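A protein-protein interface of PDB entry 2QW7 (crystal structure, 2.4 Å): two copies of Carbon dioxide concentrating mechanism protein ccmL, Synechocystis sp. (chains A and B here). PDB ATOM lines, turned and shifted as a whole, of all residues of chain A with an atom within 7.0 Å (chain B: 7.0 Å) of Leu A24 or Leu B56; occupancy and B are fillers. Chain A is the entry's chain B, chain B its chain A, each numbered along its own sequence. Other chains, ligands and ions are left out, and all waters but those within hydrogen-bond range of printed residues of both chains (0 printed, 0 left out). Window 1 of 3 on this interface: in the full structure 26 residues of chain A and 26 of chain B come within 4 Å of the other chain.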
ATOM      1  N   GLY A   8      31.575   5.167  35.637  1.00  0.00           N
ATOM      2  CA  GLY A   8      30.150   5.154  35.426  1.00  0.00           C
ATOM      3  C   GLY A   8      29.661   3.753  35.238  1.00  0.00           C
ATOM      4  O   GLY A   8      30.306   2.841  35.749  1.00  0.00           O
ATOM      5  N   THR A   9      28.529   3.613  34.516  1.00  0.00           N
ATOM      6  CA  THR A   9      27.827   2.317  34.270  1.00  0.00           C
ATOM      7  C   THR A   9      27.564   2.006  32.793  1.00  0.00           C
ATOM      8  O   THR A   9      27.430   2.921  31.959  1.00  0.00           O
ATOM      9  CB  THR A   9      26.512   2.337  34.979  1.00  0.00           C
ATOM     10  OG1 THR A   9      26.767   2.089  36.373  1.00  0.00           O
ATOM     11  CG2 THR A   9      25.626   1.240  34.444  1.00  0.00           C
ATOM     12  N   VAL A  10      27.552   0.718  32.467  1.00  0.00           N
ATOM     13  CA  VAL A  10      27.302   0.278  31.087  1.00  0.00           C
ATOM     14  C   VAL A  10      26.000  -0.506  31.000  1.00  0.00           C
ATOM     15  O   VAL A  10      25.868  -1.546  31.643  1.00  0.00           O
ATOM     16  CB  VAL A  10      28.480  -0.592  30.469  1.00  0.00           C
ATOM     17  CG1 VAL A  10      27.942  -1.683  29.485  1.00  0.00           C
ATOM     18  CG2 VAL A  10      29.547   0.344  29.753  1.00  0.00           C
ATOM     19  N   VAL A  11      25.062  -0.018  30.197  1.00  0.00           N
ATOM     20  CA  VAL A  11      23.809  -0.683  30.002  1.00  0.00           C
ATOM     21  C   VAL A  11      23.880  -1.429  28.670  1.00  0.00           C
ATOM     22  O   VAL A  11      24.280  -0.874  27.651  1.00  0.00           O
ATOM     23  CB  VAL A  11      22.622   0.338  29.962  1.00  0.00           C
ATOM     24  CG1 VAL A  11      21.353  -0.233  29.331  1.00  0.00           C
ATOM     25  CG2 VAL A  11      22.354   0.904  31.340  1.00  0.00           C
ATOM     26  N   SER A  12      23.486  -2.703  28.710  1.00  0.00           N
ATOM     27  CA  SER A  12      23.438  -3.568  27.546  1.00  0.00           C
ATOM     28  C   SER A  12      22.182  -4.338  27.731  1.00  0.00           C
ATOM     29  O   SER A  12      21.996  -4.902  28.783  1.00  0.00           O
ATOM     30  CB  SER A  12      24.634  -4.566  27.468  1.00  0.00           C
ATOM     31  OG  SER A  12      24.401  -5.727  26.637  1.00  0.00           O
ATOM     32  N   LYS A  15      22.298  -8.991  25.073  1.00  0.00           N
ATOM     33  CA  LYS A  15      23.456  -9.692  25.629  1.00  0.00           C
ATOM     34  C   LYS A  15      23.236 -11.173  25.955  1.00  0.00           C
ATOM     35  O   LYS A  15      22.124 -11.714  25.872  1.00  0.00           O
ATOM     36  CB  LYS A  15      24.007  -8.961  26.854  1.00  0.00           C
ATOM     37  CG  LYS A  15      23.026  -8.517  27.892  1.00  0.00           C
ATOM     38  CD  LYS A  15      23.741  -7.672  28.999  1.00  0.00           C
ATOM     39  CE  LYS A  15      22.726  -7.362  30.139  1.00  0.00           C
ATOM     40  NZ  LYS A  15      23.377  -7.106  31.445  1.00  0.00           N
ATOM     41  N   LEU A  19      25.168 -13.100  31.195  1.00  0.00           N
ATOM     42  CA  LEU A  19      25.465 -11.766  31.691  1.00  0.00           C
ATOM     43  C   LEU A  19      24.221 -11.123  32.279  1.00  0.00           C
ATOM     44  O   LEU A  19      24.228  -9.891  32.503  1.00  0.00           O
ATOM     45  CB  LEU A  19      25.951 -10.836  30.593  1.00  0.00           C
ATOM     46  CG  LEU A  19      27.402 -10.455  30.516  1.00  0.00           C
ATOM     47  CD1 LEU A  19      28.274 -11.593  31.002  1.00  0.00           C
ATOM     48  CD2 LEU A  19      27.786  -9.924  29.107  1.00  0.00           C
ATOM     49  N   GLY A  21      21.761 -10.203  35.119  1.00  0.00           N
ATOM     50  CA  GLY A  21      21.888 -10.098  36.567  1.00  0.00           C
ATOM     51  C   GLY A  21      23.254  -9.602  37.013  1.00  0.00           C
ATOM     52  O   GLY A  21      23.495  -9.481  38.201  1.00  0.00           O
ATOM     53  N   VAL A  22      24.150  -9.294  36.069  1.00  0.00           N
ATOM     54  CA  VAL A  22      25.444  -8.710  36.470  1.00  0.00           C
ATOM     55  C   VAL A  22      25.468  -7.201  36.207  1.00  0.00           C
ATOM     56  O   VAL A  22      25.157  -6.743  35.099  1.00  0.00           O
ATOM     57  CB  VAL A  22      26.743  -9.494  36.036  1.00  0.00           C
ATOM     58  CG1 VAL A  22      26.771  -9.915  34.597  1.00  0.00           C
ATOM     59  CG2 VAL A  22      27.990  -8.669  36.365  1.00  0.00           C
ATOM     60  N   LYS A  23      25.808  -6.450  37.252  1.00  0.00           N
ATOM     61  CA  LYS A  23      25.965  -4.977  37.205  1.00  0.00           C
ATOM     62  C   LYS A  23      27.282  -4.650  36.450  1.00  0.00           C
ATOM     63  O   LYS A  23      28.340  -5.126  36.786  1.00  0.00           O
ATOM     64  CB  LYS A  23      25.963  -4.443  38.650  1.00  0.00           C
ATOM     65  CG  LYS A  23      25.591  -2.988  38.894  1.00  0.00           C
ATOM     66  CD  LYS A  23      26.728  -1.960  38.682  1.00  0.00           C
ATOM     67  CE  LYS A  23      26.227  -0.499  38.819  1.00  0.00           C
ATOM     68  NZ  LYS A  23      25.482  -0.039  40.050  1.00  0.00           N
ATOM     69  N   LEU A  24      27.235  -3.855  35.411  1.00  0.00           N
ATOM     70  CA  LEU A  24      28.436  -3.580  34.614  1.00  0.00           C
ATOM     71  C   LEU A  24      28.979  -2.196  34.851  1.00  0.00           C
ATOM     72  O   LEU A  24      28.373  -1.236  34.429  1.00  0.00           O
ATOM     73  CB  LEU A  24      28.157  -3.697  33.074  1.00  0.00           C
ATOM     74  CG  LEU A  24      28.171  -5.013  32.281  1.00  0.00           C
ATOM     75  CD1 LEU A  24      27.879  -6.267  33.208  1.00  0.00           C
ATOM     76  CD2 LEU A  24      27.163  -4.804  31.086  1.00  0.00           C
ATOM     77  N   LEU A  25      30.155  -2.103  35.446  1.00  0.00           N
ATOM     78  CA  LEU A  25      30.766  -0.794  35.702  1.00  0.00           C
ATOM     79  C   LEU A  25      31.970  -0.535  34.872  1.00  0.00           C
ATOM     80  O   LEU A  25      32.880  -1.387  34.844  1.00  0.00           O
ATOM     81  CB  LEU A  25      31.305  -0.636  37.111  1.00  0.00           C
ATOM     82  CG  LEU A  25      30.276  -0.472  38.187  1.00  0.00           C
ATOM     83  CD1 LEU A  25      31.089  -0.032  39.409  1.00  0.00           C
ATOM     84  CD2 LEU A  25      29.221   0.512  37.672  1.00  0.00           C
ATOM     85  N   LEU A  26      32.001   0.683  34.326  1.00  0.00           N
ATOM     86  CA  LEU A  26      33.187   1.195  33.626  1.00  0.00           C
ATOM     87  C   LEU A  26      34.163   1.671  34.686  1.00  0.00           C
ATOM     88  O   LEU A  26      33.857   2.626  35.375  1.00  0.00           O
ATOM     89  CB  LEU A  26      32.862   2.398  32.721  1.00  0.00           C
ATOM     90  CG  LEU A  26      34.049   3.151  32.064  1.00  0.00           C
ATOM     91  CD1 LEU A  26      34.694   2.265  30.998  1.00  0.00           C
ATOM     92  CD2 LEU A  26      33.700   4.502  31.417  1.00  0.00           C
ATOM     93  N   VAL A  42      35.382  -2.797  31.619  1.00  0.00           N
ATOM     94  CA  VAL A  42      33.991  -2.763  31.933  1.00  0.00           C
ATOM     95  C   VAL A  42      33.951  -4.066  32.729  1.00  0.00           C
ATOM     96  O   VAL A  42      34.197  -5.155  32.173  1.00  0.00           O
ATOM     97  CB  VAL A  42      33.042  -2.699  30.728  1.00  0.00           C
ATOM     98  CG1 VAL A  42      31.679  -2.845  31.194  1.00  0.00           C
ATOM     99  CG2 VAL A  42      33.194  -1.315  29.969  1.00  0.00           C
ATOM    100  N   ALA A  43      33.769  -3.925  34.047  1.00  0.00           N
ATOM    101  CA  ALA A  43      33.761  -5.083  34.976  1.00  0.00           C
ATOM    102  C   ALA A  43      32.466  -5.256  35.725  1.00  0.00           C
ATOM    103  O   ALA A  43      31.763  -4.295  36.035  1.00  0.00           O
ATOM    104  CB  ALA A  43      34.847  -5.006  35.990  1.00  0.00           C
ATOM    105  N   GLY A  44      32.186  -6.516  36.042  1.00  0.00           N
ATOM    106  CA  GLY A  44      31.025  -6.912  36.809  1.00  0.00           C
ATOM    107  C   GLY A  44      31.271  -6.530  38.254  1.00  0.00           C
ATOM    108  O   GLY A  44      32.358  -6.656  38.786  1.00  0.00           O
ATOM    109  N   ASP A  45      30.251  -6.059  38.936  1.00  0.00           N
ATOM    110  CA  ASP A  45      30.472  -5.563  40.290  1.00  0.00           C
ATOM    111  C   ASP A  45      29.726  -6.412  41.287  1.00  0.00           C
ATOM    112  O   ASP A  45      28.522  -6.476  41.276  1.00  0.00           O
ATOM    113  CB  ASP A  45      30.139  -4.068  40.390  1.00  0.00           C
ATOM    114  CG  ASP A  45      30.332  -3.528  41.806  1.00  0.00           C
ATOM    115  OD1 ASP A  45      30.661  -4.326  42.750  1.00  0.00           O
ATOM    116  OD2 ASP A  45      30.119  -2.291  41.958  1.00  0.00           O
ATOM    117  N   LEU A  74      32.951 -13.278  32.257  1.00  0.00           N
ATOM    118  CA  LEU A  74      33.631 -12.073  32.842  1.00  0.00           C
ATOM    119  C   LEU A  74      35.116 -12.131  32.816  1.00  0.00           C
ATOM    120  O   LEU A  74      35.776 -13.073  33.247  1.00  0.00           O
ATOM    121  CB  LEU A  74      33.193 -11.627  34.245  1.00  0.00           C
ATOM    122  CG  LEU A  74      31.703 -11.312  34.258  1.00  0.00           C
ATOM    123  CD1 LEU A  74      31.019 -11.830  35.530  1.00  0.00           C
ATOM    124  CD2 LEU A  74      31.530  -9.850  33.898  1.00  0.00           C
ATOM    125  N   MET B   1      35.714  -6.639  30.808  1.00  0.00           N
ATOM    126  CA  MET B   1      35.466  -6.598  29.328  1.00  0.00           C
ATOM    127  C   MET B   1      35.835  -5.253  28.681  1.00  0.00           C
ATOM    128  O   MET B   1      36.151  -4.285  29.368  1.00  0.00           O
ATOM    129  CB  MET B   1      34.070  -7.111  28.952  1.00  0.00           C
ATOM    130  CG  MET B   1      32.939  -6.994  29.962  1.00  0.00           C
ATOM    131  SD  MET B   1      32.748  -8.415  31.075  1.00  0.00           S
ATOM    132  CE  MET B   1      33.953  -8.132  32.364  1.00  0.00           C
ATOM    133  N   GLN B   2      35.908  -5.220  27.347  1.00  0.00           N
ATOM    134  CA  GLN B   2      36.304  -3.976  26.635  1.00  0.00           C
ATOM    135  C   GLN B   2      35.228  -3.424  25.721  1.00  0.00           C
ATOM    136  O   GLN B   2      34.447  -4.128  25.104  1.00  0.00           O
ATOM    137  CB  GLN B   2      37.604  -4.118  25.833  1.00  0.00           C
ATOM    138  CG  GLN B   2      38.962  -4.252  26.594  1.00  0.00           C
ATOM    139  CD  GLN B   2      39.524  -3.031  27.181  1.00  0.00           C
ATOM    140  OE1 GLN B   2      40.161  -2.188  26.487  1.00  0.00           O
ATOM    141  NE2 GLN B   2      39.387  -2.919  28.493  1.00  0.00           N
ATOM    142  N   LEU B   3      35.172  -2.105  25.669  1.00  0.00           N
ATOM    143  CA  LEU B   3      34.207  -1.455  24.836  1.00  0.00           C
ATOM    144  C   LEU B   3      34.932  -1.495  23.472  1.00  0.00           C
ATOM    145  O   LEU B   3      36.145  -1.293  23.417  1.00  0.00           O
ATOM    146  CB  LEU B   3      33.900  -0.050  25.320  1.00  0.00           C
ATOM    147  CG  LEU B   3      33.368   0.376  26.699  1.00  0.00           C
ATOM    148  CD1 LEU B   3      33.811   1.936  26.905  1.00  0.00           C
ATOM    149  CD2 LEU B   3      31.874   0.116  26.900  1.00  0.00           C
ATOM    150  N   ALA B   4      34.171  -1.789  22.418  1.00  0.00           N
ATOM    151  CA  ALA B   4      34.657  -1.948  21.069  1.00  0.00           C
ATOM    152  C   ALA B   4      33.577  -1.644  20.049  1.00  0.00           C
ATOM    153  O   ALA B   4      32.384  -1.731  20.354  1.00  0.00           O
ATOM    154  CB  ALA B   4      35.123  -3.309  20.849  1.00  0.00           C
ATOM    155  N   VAL B  47      25.876 -12.745  19.957  1.00  0.00           N
ATOM    156  CA  VAL B  47      24.850 -11.760  20.248  1.00  0.00           C
ATOM    157  C   VAL B  47      24.177 -11.107  18.986  1.00  0.00           C
ATOM    158  O   VAL B  47      23.039 -10.614  19.030  1.00  0.00           O
ATOM    159  CB  VAL B  47      25.520 -10.803  21.331  1.00  0.00           C
ATOM    160  CG1 VAL B  47      25.599  -9.300  20.976  1.00  0.00           C
ATOM    161  CG2 VAL B  47      24.952 -11.064  22.681  1.00  0.00           C
ATOM    162  N   TRP B  54      28.510  -0.474  18.924  1.00  0.00           N
ATOM    163  CA  TRP B  54      29.393  -0.551  20.091  1.00  0.00           C
ATOM    164  C   TRP B  54      29.021  -1.803  20.841  1.00  0.00           C
ATOM    165  O   TRP B  54      27.834  -2.075  21.091  1.00  0.00           O
ATOM    166  CB  TRP B  54      29.225   0.614  21.045  1.00  0.00           C
ATOM    167  CG  TRP B  54      29.855   1.856  20.613  1.00  0.00           C
ATOM    168  CD1 TRP B  54      30.005   2.312  19.333  1.00  0.00           C
ATOM    169  CD2 TRP B  54      30.416   2.860  21.464  1.00  0.00           C
ATOM    170  NE1 TRP B  54      30.659   3.548  19.334  1.00  0.00           N
ATOM    171  CE2 TRP B  54      30.921   3.893  20.633  1.00  0.00           C
ATOM    172  CE3 TRP B  54      30.560   2.980  22.844  1.00  0.00           C
ATOM    173  CZ2 TRP B  54      31.524   5.035  21.147  1.00  0.00           C
ATOM    174  CZ3 TRP B  54      31.172   4.110  23.348  1.00  0.00           C
ATOM    175  CH2 TRP B  54      31.643   5.120  22.502  1.00  0.00           C
ATOM    176  N   VAL B  55      30.052  -2.536  21.270  1.00  0.00           N
ATOM    177  CA  VAL B  55      29.862  -3.852  21.843  1.00  0.00           C
ATOM    178  C   VAL B  55      30.777  -4.137  23.032  1.00  0.00           C
ATOM    179  O   VAL B  55      31.782  -3.458  23.269  1.00  0.00           O
ATOM    180  CB  VAL B  55      30.062  -4.887  20.667  1.00  0.00           C
ATOM    181  CG1 VAL B  55      29.310  -4.414  19.376  1.00  0.00           C
ATOM    182  CG2 VAL B  55      31.503  -5.072  20.320  1.00  0.00           C
ATOM    183  N   LEU B  56      30.395  -5.177  23.781  1.00  0.00           N
ATOM    184  CA  LEU B  56      31.186  -5.684  24.917  1.00  0.00           C
ATOM    185  C   LEU B  56      31.950  -6.900  24.496  1.00  0.00           C
ATOM    186  O   LEU B  56      31.318  -7.897  24.121  1.00  0.00           O
ATOM    187  CB  LEU B  56      30.325  -6.140  26.078  1.00  0.00           C
ATOM    188  CG  LEU B  56      29.667  -4.895  26.638  1.00  0.00           C
ATOM    189  CD1 LEU B  56      28.970  -5.454  27.875  1.00  0.00           C
ATOM    190  CD2 LEU B  56      30.655  -3.627  26.812  1.00  0.00           C
ATOM    191  N   VAL B  57      33.281  -6.830  24.692  1.00  0.00           N
ATOM    192  CA  VAL B  57      34.227  -7.885  24.302  1.00  0.00           C
ATOM    193  C   VAL B  57      34.806  -8.575  25.528  1.00  0.00           C
ATOM    194  O   VAL B  57      35.478  -7.952  26.326  1.00  0.00           O
ATOM    195  CB  VAL B  57      35.475  -7.250  23.530  1.00  0.00           C
ATOM    196  CG1 VAL B  57      36.430  -8.349  23.119  1.00  0.00           C
ATOM    197  CG2 VAL B  57      35.064  -6.283  22.276  1.00  0.00           C
ATOM    198  N   ALA B  58      34.524  -9.842  25.699  1.00  0.00           N
ATOM    199  CA  ALA B  58      35.112 -10.642  26.738  1.00  0.00           C
ATOM    200  C   ALA B  58      36.403 -11.263  26.213  1.00  0.00           C
ATOM    201  O   ALA B  58      36.398 -11.908  25.182  1.00  0.00           O
ATOM    202  CB  ALA B  58      34.117 -11.788  27.195  1.00  0.00           C
ATOM    203  N   MET B  77      35.232 -12.855  22.624  1.00  0.00           N
ATOM    204  CA  MET B  77      33.831 -13.061  22.360  1.00  0.00           C
ATOM    205  C   MET B  77      33.049 -11.784  22.550  1.00  0.00           C
ATOM    206  O   MET B  77      33.218 -11.108  23.549  1.00  0.00           O
ATOM    207  CB  MET B  77      33.296 -14.115  23.389  1.00  0.00           C
ATOM    208  CG  MET B  77      31.857 -14.450  23.146  1.00  0.00           C
ATOM    209  SD  MET B  77      31.711 -15.243  21.496  1.00  0.00           S
ATOM    210  CE  MET B  77      31.295 -16.949  21.930  1.00  0.00           C
ATOM    211  N   VAL B  78      32.153 -11.500  21.606  1.00  0.00           N
ATOM    212  CA  VAL B  78      31.204 -10.356  21.680  1.00  0.00           C
ATOM    213  C   VAL B  78      30.017 -10.886  22.493  1.00  0.00           C
ATOM    214  O   VAL B  78      29.276 -11.804  22.059  1.00  0.00           O
ATOM    215  CB  VAL B  78      30.744  -9.914  20.323  1.00  0.00           C
ATOM    216  CG1 VAL B  78      29.588  -9.020  20.468  1.00  0.00           C
ATOM    217  CG2 VAL B  78      31.918  -9.244  19.583  1.00  0.00           C
ATOM    218  N   VAL B  79      29.951 -10.388  23.729  1.00  0.00           N
ATOM    219  CA  VAL B  79      29.013 -10.891  24.769  1.00  0.00           C
ATOM    220  C   VAL B  79      27.828  -9.937  24.984  1.00  0.00           C
ATOM    221  O   VAL B  79      26.912 -10.266  25.725  1.00  0.00           O
ATOM    222  CB  VAL B  79      29.780 -11.168  26.065  1.00  0.00           C
ATOM    223  CG1 VAL B  79      30.755 -12.308  25.849  1.00  0.00           C
ATOM    224  CG2 VAL B  79      30.604  -9.912  26.529  1.00  0.00           C
ATOM    225  N   GLY B  80      27.869  -8.765  24.299  1.00  0.00           N
ATOM    226  CA  GLY B  80      26.726  -7.852  24.314  1.00  0.00           C
ATOM    227  C   GLY B  80      26.836  -6.573  23.521  1.00  0.00           C
ATOM    228  O   GLY B  80      27.940  -6.108  23.201  1.00  0.00           O
ATOM    229  N   ILE B  81      25.672  -6.001  23.202  1.00  0.00           N
ATOM    230  CA  ILE B  81      25.638  -4.735  22.450  1.00  0.00           C
ATOM    231  C   ILE B  81      25.314  -3.646  23.484  1.00  0.00           C
ATOM    232  O   ILE B  81      24.424  -3.817  24.344  1.00  0.00           O
ATOM    233  CB  ILE B  81      24.731  -4.627  21.137  1.00  0.00           C
ATOM    234  CG1 ILE B  81      24.935  -5.805  20.173  1.00  0.00           C
ATOM    235  CG2 ILE B  81      25.122  -3.336  20.352  1.00  0.00           C
ATOM    236  CD1 ILE B  81      23.920  -5.792  19.020  1.00  0.00           C
ATOM    237  N   ILE B  82      26.040  -2.524  23.342  1.00  0.00           N
ATOM    238  CA  ILE B  82      25.949  -1.448  24.300  1.00  0.00           C
ATOM    239  C   ILE B  82      24.861  -0.472  23.912  1.00  0.00           C
ATOM    240  O   ILE B  82      24.821  -0.027  22.771  1.00  0.00           O
ATOM    241  CB  ILE B  82      27.325  -0.750  24.511  1.00  0.00           C
ATOM    242  CG1 ILE B  82      28.352  -1.787  24.918  1.00  0.00           C
ATOM    243  CG2 ILE B  82      27.270   0.321  25.654  1.00  0.00           C
ATOM    244  CD1 ILE B  82      29.698  -1.315  24.766  1.00  0.00           C
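The backbone NH of Met B1 lies within hydrogen-bond range of the backbone carbonyl oxygen of Val A42, 2.5 Å away. The backbone carbonyl oxygen (O) of Ile B81 sits at hydrogen-bond distance from the side-chain hydroxyl (OG) of Ser A12 (3.0 Å).
Printed residues of chain A that touch a printed residue of chain B: Val A10, Val A11, Ser A12, Lys A15, Leu A19, Leu A24, Val A42 and Leu A74. Hydrophobic or aromatic side chains of chain B within 4 Å of the printed part of chain A: Met B1, Leu B3, Val B47, Leu B56, Val B79 and Ile B82. Among the printed residues, 12 pairs touch across the chains.
Among the printed residues, merely in contact across the chains: Val A10 with Leu B3, Val A11 with Ile B82, Ser A12 with Gly B80, Lys A15 with Val B47, Lys A15 with Val B79, Lys A15 with Gly B80, Leu A19 with Val B79, Leu A24 with Leu B56, Val A42 with Leu B3 and Leu A74 with Met B1.
The backbone NH of Ile B82 sits at hydrogen-bond distance from the backbone carbonyl oxygen of Trp B54 (2.9 Å). The backbone carbonyl oxygen of Leu B56 is in hydrogen-bond range of the backbone NH of Val B79. The backbone NH (N) of Leu B56 lies within hydrogen-bond range of the backbone carbonyl oxygen (O) of Gly B80 (2.7 Å). The backbone NH (N) of Val A10 is in hydrogen-bond range of the backbone carbonyl oxygen (O) of Leu A24, 2.9 Å away. The side-chain amino group of Lys A15 sits at hydrogen-bond distance from the backbone carbonyl oxygen of Leu A19, at 3.1 Å.
No position is printed for both chains. Of the 12 pairs that touch across the chains among the printed residues, none has its exchanged pair printed and touching as well.
Of the printed residues of chain B, Ser A12 touches Gly B80 (3.9 Å) and Ile B81 (3.0 Å). Leu A24 touches one residue of chain B. Of the printed residues of chain B, Val A42 touches Met B1 (2.5 Å) and Leu B3 (3.6 Å). Of the printed residues of chain A, Val B47 touches Lys A15 (3.6 Å). Printed residues of chain A within 4 Å of Leu B56: Leu A24 (3.7 Å). Met B77 touches none of the printed residues of chain A. Of the printed residues of chain A, Ile B81 touches Ser A12. The nearest printed residue of chain B that does not touch Leu A24 is Met B1 (5.7 Å). The nearest residue of chain A that does not touch Leu B56 is Val A10 (4.2 Å). The nearest printed residue of chain B that does not touch Val A10 is Leu B56 (4.2 Å).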
